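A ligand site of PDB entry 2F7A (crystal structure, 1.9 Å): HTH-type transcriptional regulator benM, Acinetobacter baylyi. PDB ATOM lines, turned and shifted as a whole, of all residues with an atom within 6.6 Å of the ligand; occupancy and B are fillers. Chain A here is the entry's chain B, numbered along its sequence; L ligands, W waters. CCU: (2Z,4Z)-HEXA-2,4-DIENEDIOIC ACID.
An oxygen (O3) of the ligand lies within hydrogen-bond range of the backbone NH of Phe 123 (2.8 Å). N of Ser 19 lies within hydrogen-bond range of O2 of the ligand (3.0 Å). NE of Arg 66 lies within salt-bridge range of O1 of the ligand (3.6 Å). The side-chain hydroxyl of Thr 48 lies within hydrogen-bond range of an oxygen (O4) of the ligand, 2.9 Å away. The side-chain hydroxyl of Ser 19 lies within hydrogen-bond range of an oxygen (O1) of the ligand (2.4 Å). O4 of the ligand is in hydrogen-bond range of N of Thr 48, at 3.2 Å.
OG1 of Thr 125 lies within hydrogen-bond range of N of Asn 122. The guanidinium group (NE) of Arg 66 sits at hydrogen-bond distance from the side-chain hydroxyl (OG) of Ser 19, 3.0 Å away. The side-chain hydroxyl of Ser 124 sits at hydrogen-bond distance from the side-chain amide oxygen of Asn 122 (2.6 Å). The backbone carbonyl oxygen (O) of Tyr 115 is in hydrogen-bond range of the backbone NH (N) of Ser 124. OG1 of Thr 48 is in hydrogen-bond range of N of Arg 66 (3.2 Å). The guanidinium group of Arg 66 sits at hydrogen-bond distance from the side-chain hydroxyl of Thr 187, 3.1 Å away. O of Pro 119 is in hydrogen-bond range of ND2 of Asn 122, 3.5 Å away. The side-chain amide nitrogen of Asn 122 lies within hydrogen-bond range of the backbone carbonyl oxygen of Ser 118, 2.9 Å away.
Merely in contact with the ligand: Val 17, Gly 18, Leu 67, Tyr 115, Pro 116 and Asn 122. Hydrophobic or aromatic side chains within 4 Å of the ligand: Val 17, Leu 67, Tyr 115, Pro 116 and Phe 123. The nearest printed residue that does not touch the ligand is Gly 47 (4.1 Å).
Water W4 lies within hydrogen-bond range of O1 of the ligand (2.7 Å) and OH of Tyr 115 (2.9 Å). Water W3 lies within hydrogen-bond range of the backbone carbonyl oxygen of Pro 121, an oxygen (O4) of the ligand, the backbone NH of Lys 49 and the backbone NH of Thr 48. Water W2 bridges an oxygen (O3) of the ligand and the side-chain hydroxyl (OG) of Ser 118. Water W1 lies within hydrogen-bond range of an oxygen (O2) of the ligand and the backbone NH of Val 147.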
ATOM      1  N   VAL A  17      14.900 -23.560  -0.667  1.00  0.00           N
ATOM      2  CA  VAL A  17      15.419 -24.036  -1.947  1.00  0.00           C
ATOM      3  C   VAL A  17      15.028 -25.509  -2.161  1.00  0.00           C
ATOM      4  O   VAL A  17      15.000 -26.311  -1.218  1.00  0.00           O
ATOM      5  CB  VAL A  17      16.949 -23.811  -2.073  1.00  0.00           C
ATOM      6  CG1 VAL A  17      17.303 -22.317  -2.005  1.00  0.00           C
ATOM      7  CG2 VAL A  17      17.744 -24.604  -1.021  1.00  0.00           C
ATOM      8  N   GLY A  18      14.713 -25.858  -3.403  1.00  0.00           N
ATOM      9  CA  GLY A  18      14.111 -27.168  -3.733  1.00  0.00           C
ATOM     10  C   GLY A  18      14.806 -28.390  -3.157  1.00  0.00           C
ATOM     11  O   GLY A  18      14.145 -29.307  -2.659  1.00  0.00           O
ATOM     12  N   SER A  19      16.140 -28.402  -3.237  1.00  0.00           N
ATOM     13  CA  SER A  19      16.928 -29.551  -2.783  1.00  0.00           C
ATOM     14  C   SER A  19      16.629 -29.981  -1.350  1.00  0.00           C
ATOM     15  O   SER A  19      16.747 -31.164  -1.009  1.00  0.00           O
ATOM     16  CB  SER A  19      18.425 -29.256  -2.916  1.00  0.00           C
ATOM     17  OG  SER A  19      18.743 -28.024  -2.290  1.00  0.00           O
ATOM     18  N   LEU A  20      16.212 -29.026  -0.518  1.00  0.00           N
ATOM     19  CA  LEU A  20      15.931 -29.319   0.894  1.00  0.00           C
ATOM     20  C   LEU A  20      14.738 -30.261   1.079  1.00  0.00           C
ATOM     21  O   LEU A  20      14.680 -31.000   2.053  1.00  0.00           O
ATOM     22  CB  LEU A  20      15.735 -28.027   1.692  1.00  0.00           C
ATOM     23  CG  LEU A  20      16.904 -27.027   1.676  1.00  0.00           C
ATOM     24  CD1 LEU A  20      16.527 -25.740   2.394  1.00  0.00           C
ATOM     25  CD2 LEU A  20      18.167 -27.623   2.279  1.00  0.00           C
ATOM     26  N   GLU A  45       8.744 -22.507  -2.483  1.00  0.00           N
ATOM     27  CA  GLU A  45      10.037 -22.766  -3.082  1.00  0.00           C
ATOM     28  C   GLU A  45      10.547 -21.502  -3.783  1.00  0.00           C
ATOM     29  O   GLU A  45       9.848 -20.932  -4.622  1.00  0.00           O
ATOM     30  CB  GLU A  45       9.951 -23.939  -4.070  1.00  0.00           C
ATOM     31  CG  GLU A  45      11.281 -24.611  -4.363  1.00  0.00           C
ATOM     32  CD  GLU A  45      11.837 -24.288  -5.734  1.00  0.00           C
ATOM     33  OE1 GLU A  45      12.026 -23.082  -6.050  1.00  0.00           O
ATOM     34  OE2 GLU A  45      12.115 -25.243  -6.490  1.00  0.00           O
ATOM     35  N   MET A  46      11.742 -21.073  -3.421  1.00  0.00           N
ATOM     36  CA  MET A  46      12.364 -19.911  -4.050  1.00  0.00           C
ATOM     37  C   MET A  46      13.865 -19.904  -3.795  1.00  0.00           C
ATOM     38  O   MET A  46      14.342 -20.534  -2.848  1.00  0.00           O
ATOM     39  CB  MET A  46      11.732 -18.611  -3.553  1.00  0.00           C
ATOM     40  CG  MET A  46      11.621 -18.483  -2.031  1.00  0.00           C
ATOM     41  SD  MET A  46      11.058 -16.845  -1.487  1.00  0.00           S
ATOM     42  CE  MET A  46       9.335 -16.917  -1.980  1.00  0.00           C
ATOM     43  N   GLY A  47      14.606 -19.204  -4.647  1.00  0.00           N
ATOM     44  CA  GLY A  47      16.048 -19.067  -4.491  1.00  0.00           C
ATOM     45  C   GLY A  47      16.429 -18.229  -3.294  1.00  0.00           C
ATOM     46  O   GLY A  47      15.599 -17.476  -2.754  1.00  0.00           O
ATOM     47  N   THR A  48      17.695 -18.328  -2.888  1.00  0.00           N
ATOM     48  CA  THR A  48      18.193 -17.653  -1.684  1.00  0.00           C
ATOM     49  C   THR A  48      18.136 -16.122  -1.819  1.00  0.00           C
ATOM     50  O   THR A  48      17.792 -15.433  -0.857  1.00  0.00           O
ATOM     51  CB  THR A  48      19.636 -18.106  -1.342  1.00  0.00           C
ATOM     52  OG1 THR A  48      19.746 -19.536  -1.438  1.00  0.00           O
ATOM     53  CG2 THR A  48      20.019 -17.675   0.074  1.00  0.00           C
ATOM     54  N   LYS A  49      18.457 -15.596  -2.992  1.00  0.00           N
ATOM     55  CA  LYS A  49      18.387 -14.150  -3.243  1.00  0.00           C
ATOM     56  C   LYS A  49      16.934 -13.674  -3.174  1.00  0.00           C
ATOM     57  O   LYS A  49      16.639 -12.598  -2.641  1.00  0.00           O
ATOM     58  CB  LYS A  49      18.983 -13.791  -4.615  1.00  0.00           C
ATOM     59  CG  LYS A  49      19.384 -12.334  -4.789  1.00  0.00           C
ATOM     60  CD  LYS A  49      20.723 -12.040  -4.102  1.00  0.00           C
ATOM     61  CE  LYS A  49      21.279 -10.668  -4.448  1.00  0.00           C
ATOM     62  NZ  LYS A  49      22.730 -10.568  -4.068  1.00  0.00           N
ATOM     63  N   GLN A  51      14.579 -15.127  -1.449  1.00  0.00           N
ATOM     64  CA  GLN A  51      14.167 -15.225  -0.051  1.00  0.00           C
ATOM     65  C   GLN A  51      14.500 -13.954   0.731  1.00  0.00           C
ATOM     66  O   GLN A  51      13.757 -13.565   1.631  1.00  0.00           O
ATOM     67  CB  GLN A  51      14.830 -16.424   0.631  1.00  0.00           C
ATOM     68  CG  GLN A  51      14.313 -17.768   0.155  1.00  0.00           C
ATOM     69  CD  GLN A  51      15.140 -18.938   0.666  1.00  0.00           C
ATOM     70  OE1 GLN A  51      15.781 -18.856   1.709  1.00  0.00           O
ATOM     71  NE2 GLN A  51      15.116 -20.041  -0.071  1.00  0.00           N
ATOM     72  N   GLY A  65      18.194 -21.521   2.855  1.00  0.00           N
ATOM     73  CA  GLY A  65      18.934 -21.359   1.609  1.00  0.00           C
ATOM     74  C   GLY A  65      20.341 -21.899   1.646  1.00  0.00           C
ATOM     75  O   GLY A  65      20.772 -22.473   2.647  1.00  0.00           O
ATOM     76  N   ARG A  66      21.061 -21.716   0.544  1.00  0.00           N
ATOM     77  CA  ARG A  66      22.399 -22.266   0.365  1.00  0.00           C
ATOM     78  C   ARG A  66      23.387 -21.212  -0.141  1.00  0.00           C
ATOM     79  O   ARG A  66      24.431 -21.560  -0.686  1.00  0.00           O
ATOM     80  CB  ARG A  66      22.342 -23.441  -0.602  1.00  0.00           C
ATOM     81  CG  ARG A  66      21.681 -24.685  -0.051  1.00  0.00           C
ATOM     82  CD  ARG A  66      21.667 -25.788  -1.087  1.00  0.00           C
ATOM     83  NE  ARG A  66      20.986 -26.995  -0.609  1.00  0.00           N
ATOM     84  CZ  ARG A  66      21.512 -27.869   0.243  1.00  0.00           C
ATOM     85  NH1 ARG A  66      22.733 -27.690   0.748  1.00  0.00           N
ATOM     86  NH2 ARG A  66      20.814 -28.940   0.588  1.00  0.00           N
ATOM     87  N   LEU A  67      23.050 -19.939   0.049  1.00  0.00           N
ATOM     88  CA  LEU A  67      23.955 -18.842  -0.257  1.00  0.00           C
ATOM     89  C   LEU A  67      23.987 -17.874   0.911  1.00  0.00           C
ATOM     90  O   LEU A  67      22.979 -17.667   1.578  1.00  0.00           O
ATOM     91  CB  LEU A  67      23.501 -18.094  -1.513  1.00  0.00           C
ATOM     92  CG  LEU A  67      23.488 -18.804  -2.870  1.00  0.00           C
ATOM     93  CD1 LEU A  67      22.852 -17.897  -3.913  1.00  0.00           C
ATOM     94  CD2 LEU A  67      24.884 -19.195  -3.278  1.00  0.00           C
ATOM     95  N   TYR A 115      22.773 -26.122 -11.889  1.00  0.00           N
ATOM     96  CA  TYR A 115      21.388 -25.699 -11.686  1.00  0.00           C
ATOM     97  C   TYR A 115      21.375 -24.723 -10.498  1.00  0.00           C
ATOM     98  O   TYR A 115      22.334 -24.689  -9.731  1.00  0.00           O
ATOM     99  CB  TYR A 115      20.506 -26.913 -11.375  1.00  0.00           C
ATOM    100  CG  TYR A 115      20.919 -27.626 -10.117  1.00  0.00           C
ATOM    101  CD1 TYR A 115      20.394 -27.248  -8.881  1.00  0.00           C
ATOM    102  CD2 TYR A 115      21.869 -28.648 -10.143  1.00  0.00           C
ATOM    103  CE1 TYR A 115      20.781 -27.878  -7.721  1.00  0.00           C
ATOM    104  CE2 TYR A 115      22.260 -29.292  -8.970  1.00  0.00           C
ATOM    105  CZ  TYR A 115      21.712 -28.894  -7.765  1.00  0.00           C
ATOM    106  OH  TYR A 115      22.090 -29.489  -6.596  1.00  0.00           O
ATOM    107  N   PRO A 116      20.315 -23.910 -10.372  1.00  0.00           N
ATOM    108  CA  PRO A 116      19.171 -23.720 -11.257  1.00  0.00           C
ATOM    109  C   PRO A 116      19.530 -22.824 -12.446  1.00  0.00           C
ATOM    110  O   PRO A 116      20.660 -22.368 -12.527  1.00  0.00           O
ATOM    111  CB  PRO A 116      18.165 -22.998 -10.353  1.00  0.00           C
ATOM    112  CG  PRO A 116      19.023 -22.190  -9.449  1.00  0.00           C
ATOM    113  CD  PRO A 116      20.228 -23.043  -9.180  1.00  0.00           C
ATOM    114  N   SER A 118      17.671 -20.086 -12.938  1.00  0.00           N
ATOM    115  CA  SER A 118      17.152 -18.799 -12.481  1.00  0.00           C
ATOM    116  C   SER A 118      18.274 -17.768 -12.394  1.00  0.00           C
ATOM    117  O   SER A 118      19.443 -18.111 -12.520  1.00  0.00           O
ATOM    118  CB  SER A 118      16.446 -18.984 -11.120  1.00  0.00           C
ATOM    119  OG  SER A 118      17.193 -19.816 -10.261  1.00  0.00           O
ATOM    120  N   PRO A 119      17.935 -16.481 -12.187  1.00  0.00           N
ATOM    121  CA  PRO A 119      18.967 -15.440 -12.127  1.00  0.00           C
ATOM    122  C   PRO A 119      20.060 -15.698 -11.080  1.00  0.00           C
ATOM    123  O   PRO A 119      19.810 -16.306 -10.040  1.00  0.00           O
ATOM    124  CB  PRO A 119      18.174 -14.182 -11.754  1.00  0.00           C
ATOM    125  CG  PRO A 119      16.810 -14.443 -12.267  1.00  0.00           C
ATOM    126  CD  PRO A 119      16.580 -15.899 -12.045  1.00  0.00           C
ATOM    127  N   PRO A 121      23.002 -14.415  -8.262  1.00  0.00           N
ATOM    128  CA  PRO A 121      23.709 -15.606  -7.818  1.00  0.00           C
ATOM    129  C   PRO A 121      22.777 -16.727  -7.382  1.00  0.00           C
ATOM    130  O   PRO A 121      21.718 -16.466  -6.793  1.00  0.00           O
ATOM    131  CB  PRO A 121      24.502 -15.113  -6.627  1.00  0.00           C
ATOM    132  CG  PRO A 121      23.663 -14.047  -6.049  1.00  0.00           C
ATOM    133  CD  PRO A 121      22.930 -13.412  -7.194  1.00  0.00           C
ATOM    134  N   ASN A 122      23.188 -17.960  -7.652  1.00  0.00           N
ATOM    135  CA  ASN A 122      22.408 -19.153  -7.328  1.00  0.00           C
ATOM    136  C   ASN A 122      23.347 -20.334  -7.047  1.00  0.00           C
ATOM    137  O   ASN A 122      24.572 -20.164  -6.997  1.00  0.00           O
ATOM    138  CB  ASN A 122      21.427 -19.464  -8.474  1.00  0.00           C
ATOM    139  CG  ASN A 122      22.122 -19.691  -9.797  1.00  0.00           C
ATOM    140  OD1 ASN A 122      23.216 -20.248  -9.852  1.00  0.00           O
ATOM    141  ND2 ASN A 122      21.477 -19.266 -10.876  1.00  0.00           N
ATOM    142  N   PHE A 123      22.791 -21.529  -6.883  1.00  0.00           N
ATOM    143  CA  PHE A 123      23.598 -22.699  -6.530  1.00  0.00           C
ATOM    144  C   PHE A 123      24.752 -22.970  -7.493  1.00  0.00           C
ATOM    145  O   PHE A 123      25.828 -23.351  -7.060  1.00  0.00           O
ATOM    146  CB  PHE A 123      22.720 -23.956  -6.428  1.00  0.00           C
ATOM    147  CG  PHE A 123      23.484 -25.173  -6.011  1.00  0.00           C
ATOM    148  CD1 PHE A 123      23.990 -25.274  -4.717  1.00  0.00           C
ATOM    149  CD2 PHE A 123      23.704 -26.205  -6.908  1.00  0.00           C
ATOM    150  CE1 PHE A 123      24.705 -26.396  -4.335  1.00  0.00           C
ATOM    151  CE2 PHE A 123      24.413 -27.315  -6.526  1.00  0.00           C
ATOM    152  CZ  PHE A 123      24.907 -27.430  -5.244  1.00  0.00           C
ATOM    153  N   SER A 124      24.540 -22.781  -8.793  1.00  0.00           N
ATOM    154  CA  SER A 124      25.641 -22.993  -9.754  1.00  0.00           C
ATOM    155  C   SER A 124      26.794 -21.995  -9.560  1.00  0.00           C
ATOM    156  O   SER A 124      27.942 -22.349  -9.752  1.00  0.00           O
ATOM    157  CB  SER A 124      25.136 -22.994 -11.186  1.00  0.00           C
ATOM    158  OG  SER A 124      24.552 -21.764 -11.529  1.00  0.00           O
ATOM    159  N   THR A 125      26.477 -20.762  -9.180  1.00  0.00           N
ATOM    160  CA  THR A 125      27.501 -19.776  -8.851  1.00  0.00           C
ATOM    161  C   THR A 125      28.289 -20.232  -7.617  1.00  0.00           C
ATOM    162  O   THR A 125      29.518 -20.116  -7.565  1.00  0.00           O
ATOM    163  CB  THR A 125      26.878 -18.389  -8.604  1.00  0.00           C
ATOM    164  OG1 THR A 125      25.902 -18.472  -7.557  1.00  0.00           O
ATOM    165  CG2 THR A 125      26.185 -17.883  -9.852  1.00  0.00           C
ATOM    166  N   GLU A 146      16.502 -27.511 -12.399  1.00  0.00           N
ATOM    167  CA  GLU A 146      16.450 -27.980 -11.022  1.00  0.00           C
ATOM    168  C   GLU A 146      17.274 -29.259 -10.848  1.00  0.00           C
ATOM    169  O   GLU A 146      17.675 -29.887 -11.832  1.00  0.00           O
ATOM    170  CB  GLU A 146      14.985 -28.190 -10.599  1.00  0.00           C
ATOM    171  CG  GLU A 146      14.216 -29.182 -11.485  1.00  0.00           C
ATOM    172  CD  GLU A 146      12.706 -29.167 -11.256  1.00  0.00           C
ATOM    173  OE1 GLU A 146      12.187 -28.271 -10.565  1.00  0.00           O
ATOM    174  OE2 GLU A 146      12.032 -30.082 -11.786  1.00  0.00           O
ATOM    175  N   VAL A 147      17.521 -29.605  -9.589  1.00  0.00           N
ATOM    176  CA  VAL A 147      18.374 -30.735  -9.264  1.00  0.00           C
ATOM    177  C   VAL A 147      17.861 -32.076  -9.797  1.00  0.00           C
ATOM    178  O   VAL A 147      18.652 -32.890 -10.258  1.00  0.00           O
ATOM    179  CB  VAL A 147      18.641 -30.850  -7.735  1.00  0.00           C
ATOM    180  CG1 VAL A 147      17.368 -31.195  -6.955  1.00  0.00           C
ATOM    181  CG2 VAL A 147      19.742 -31.884  -7.470  1.00  0.00           C
ATOM    182  N   PRO A 164      24.161 -31.594  -3.325  1.00  0.00           N
ATOM    183  CA  PRO A 164      24.248 -31.810  -1.874  1.00  0.00           C
ATOM    184  C   PRO A 164      24.105 -33.286  -1.561  1.00  0.00           C
ATOM    185  O   PRO A 164      23.358 -33.983  -2.255  1.00  0.00           O
ATOM    186  CB  PRO A 164      23.034 -31.040  -1.329  1.00  0.00           C
ATOM    187  CG  PRO A 164      22.672 -30.079  -2.366  1.00  0.00           C
ATOM    188  CD  PRO A 164      23.013 -30.735  -3.675  1.00  0.00           C
ATOM    189  N   THR A 187      28.372 -27.417   0.697  1.00  0.00           N
ATOM    190  CA  THR A 187      27.242 -26.549   0.425  1.00  0.00           C
ATOM    191  C   THR A 187      26.564 -26.250   1.761  1.00  0.00           C
ATOM    192  O   THR A 187      25.761 -27.042   2.250  1.00  0.00           O
ATOM    193  CB  THR A 187      26.276 -27.189  -0.600  1.00  0.00           C
ATOM    194  OG1 THR A 187      25.128 -26.355  -0.756  1.00  0.00           O
ATOM    195  CG2 THR A 187      25.836 -28.612  -0.203  1.00  0.00           C
HETATM  196  C2  CCU L   1      18.489 -24.760  -5.562  1.00  0.00           C
HETATM  197  C3  CCU L   1      19.051 -23.534  -5.340  1.00  0.00           C
HETATM  198  C4  CCU L   1      19.930 -23.202  -4.237  1.00  0.00           C
HETATM  199  C6  CCU L   1      20.280 -20.828  -4.947  1.00  0.00           C
HETATM  200  O4  CCU L   1      20.121 -19.786  -4.306  1.00  0.00           O
HETATM  201  O3  CCU L   1      20.203 -20.849  -6.031  1.00  0.00           O
HETATM  202  C5  CCU L   1      20.484 -22.035  -4.047  1.00  0.00           C
HETATM  203  C1  CCU L   1      18.599 -26.007  -4.784  1.00  0.00           C
HETATM  204  O1  CCU L   1      19.393 -26.180  -3.739  1.00  0.00           O
HETATM  205  O2  CCU L   1      17.889 -26.910  -5.175  1.00  0.00           O
HETATM  206  O   HOH W   1      16.662 -27.343  -7.751  1.00  0.00           O
HETATM  207  O   HOH W   2      18.240 -19.313  -7.138  1.00  0.00           O
HETATM  208  O   HOH W   3      19.754 -17.262  -5.204  1.00  0.00           O
HETATM  209  O   HOH W   4      21.572 -27.565  -4.429  1.00  0.00           O
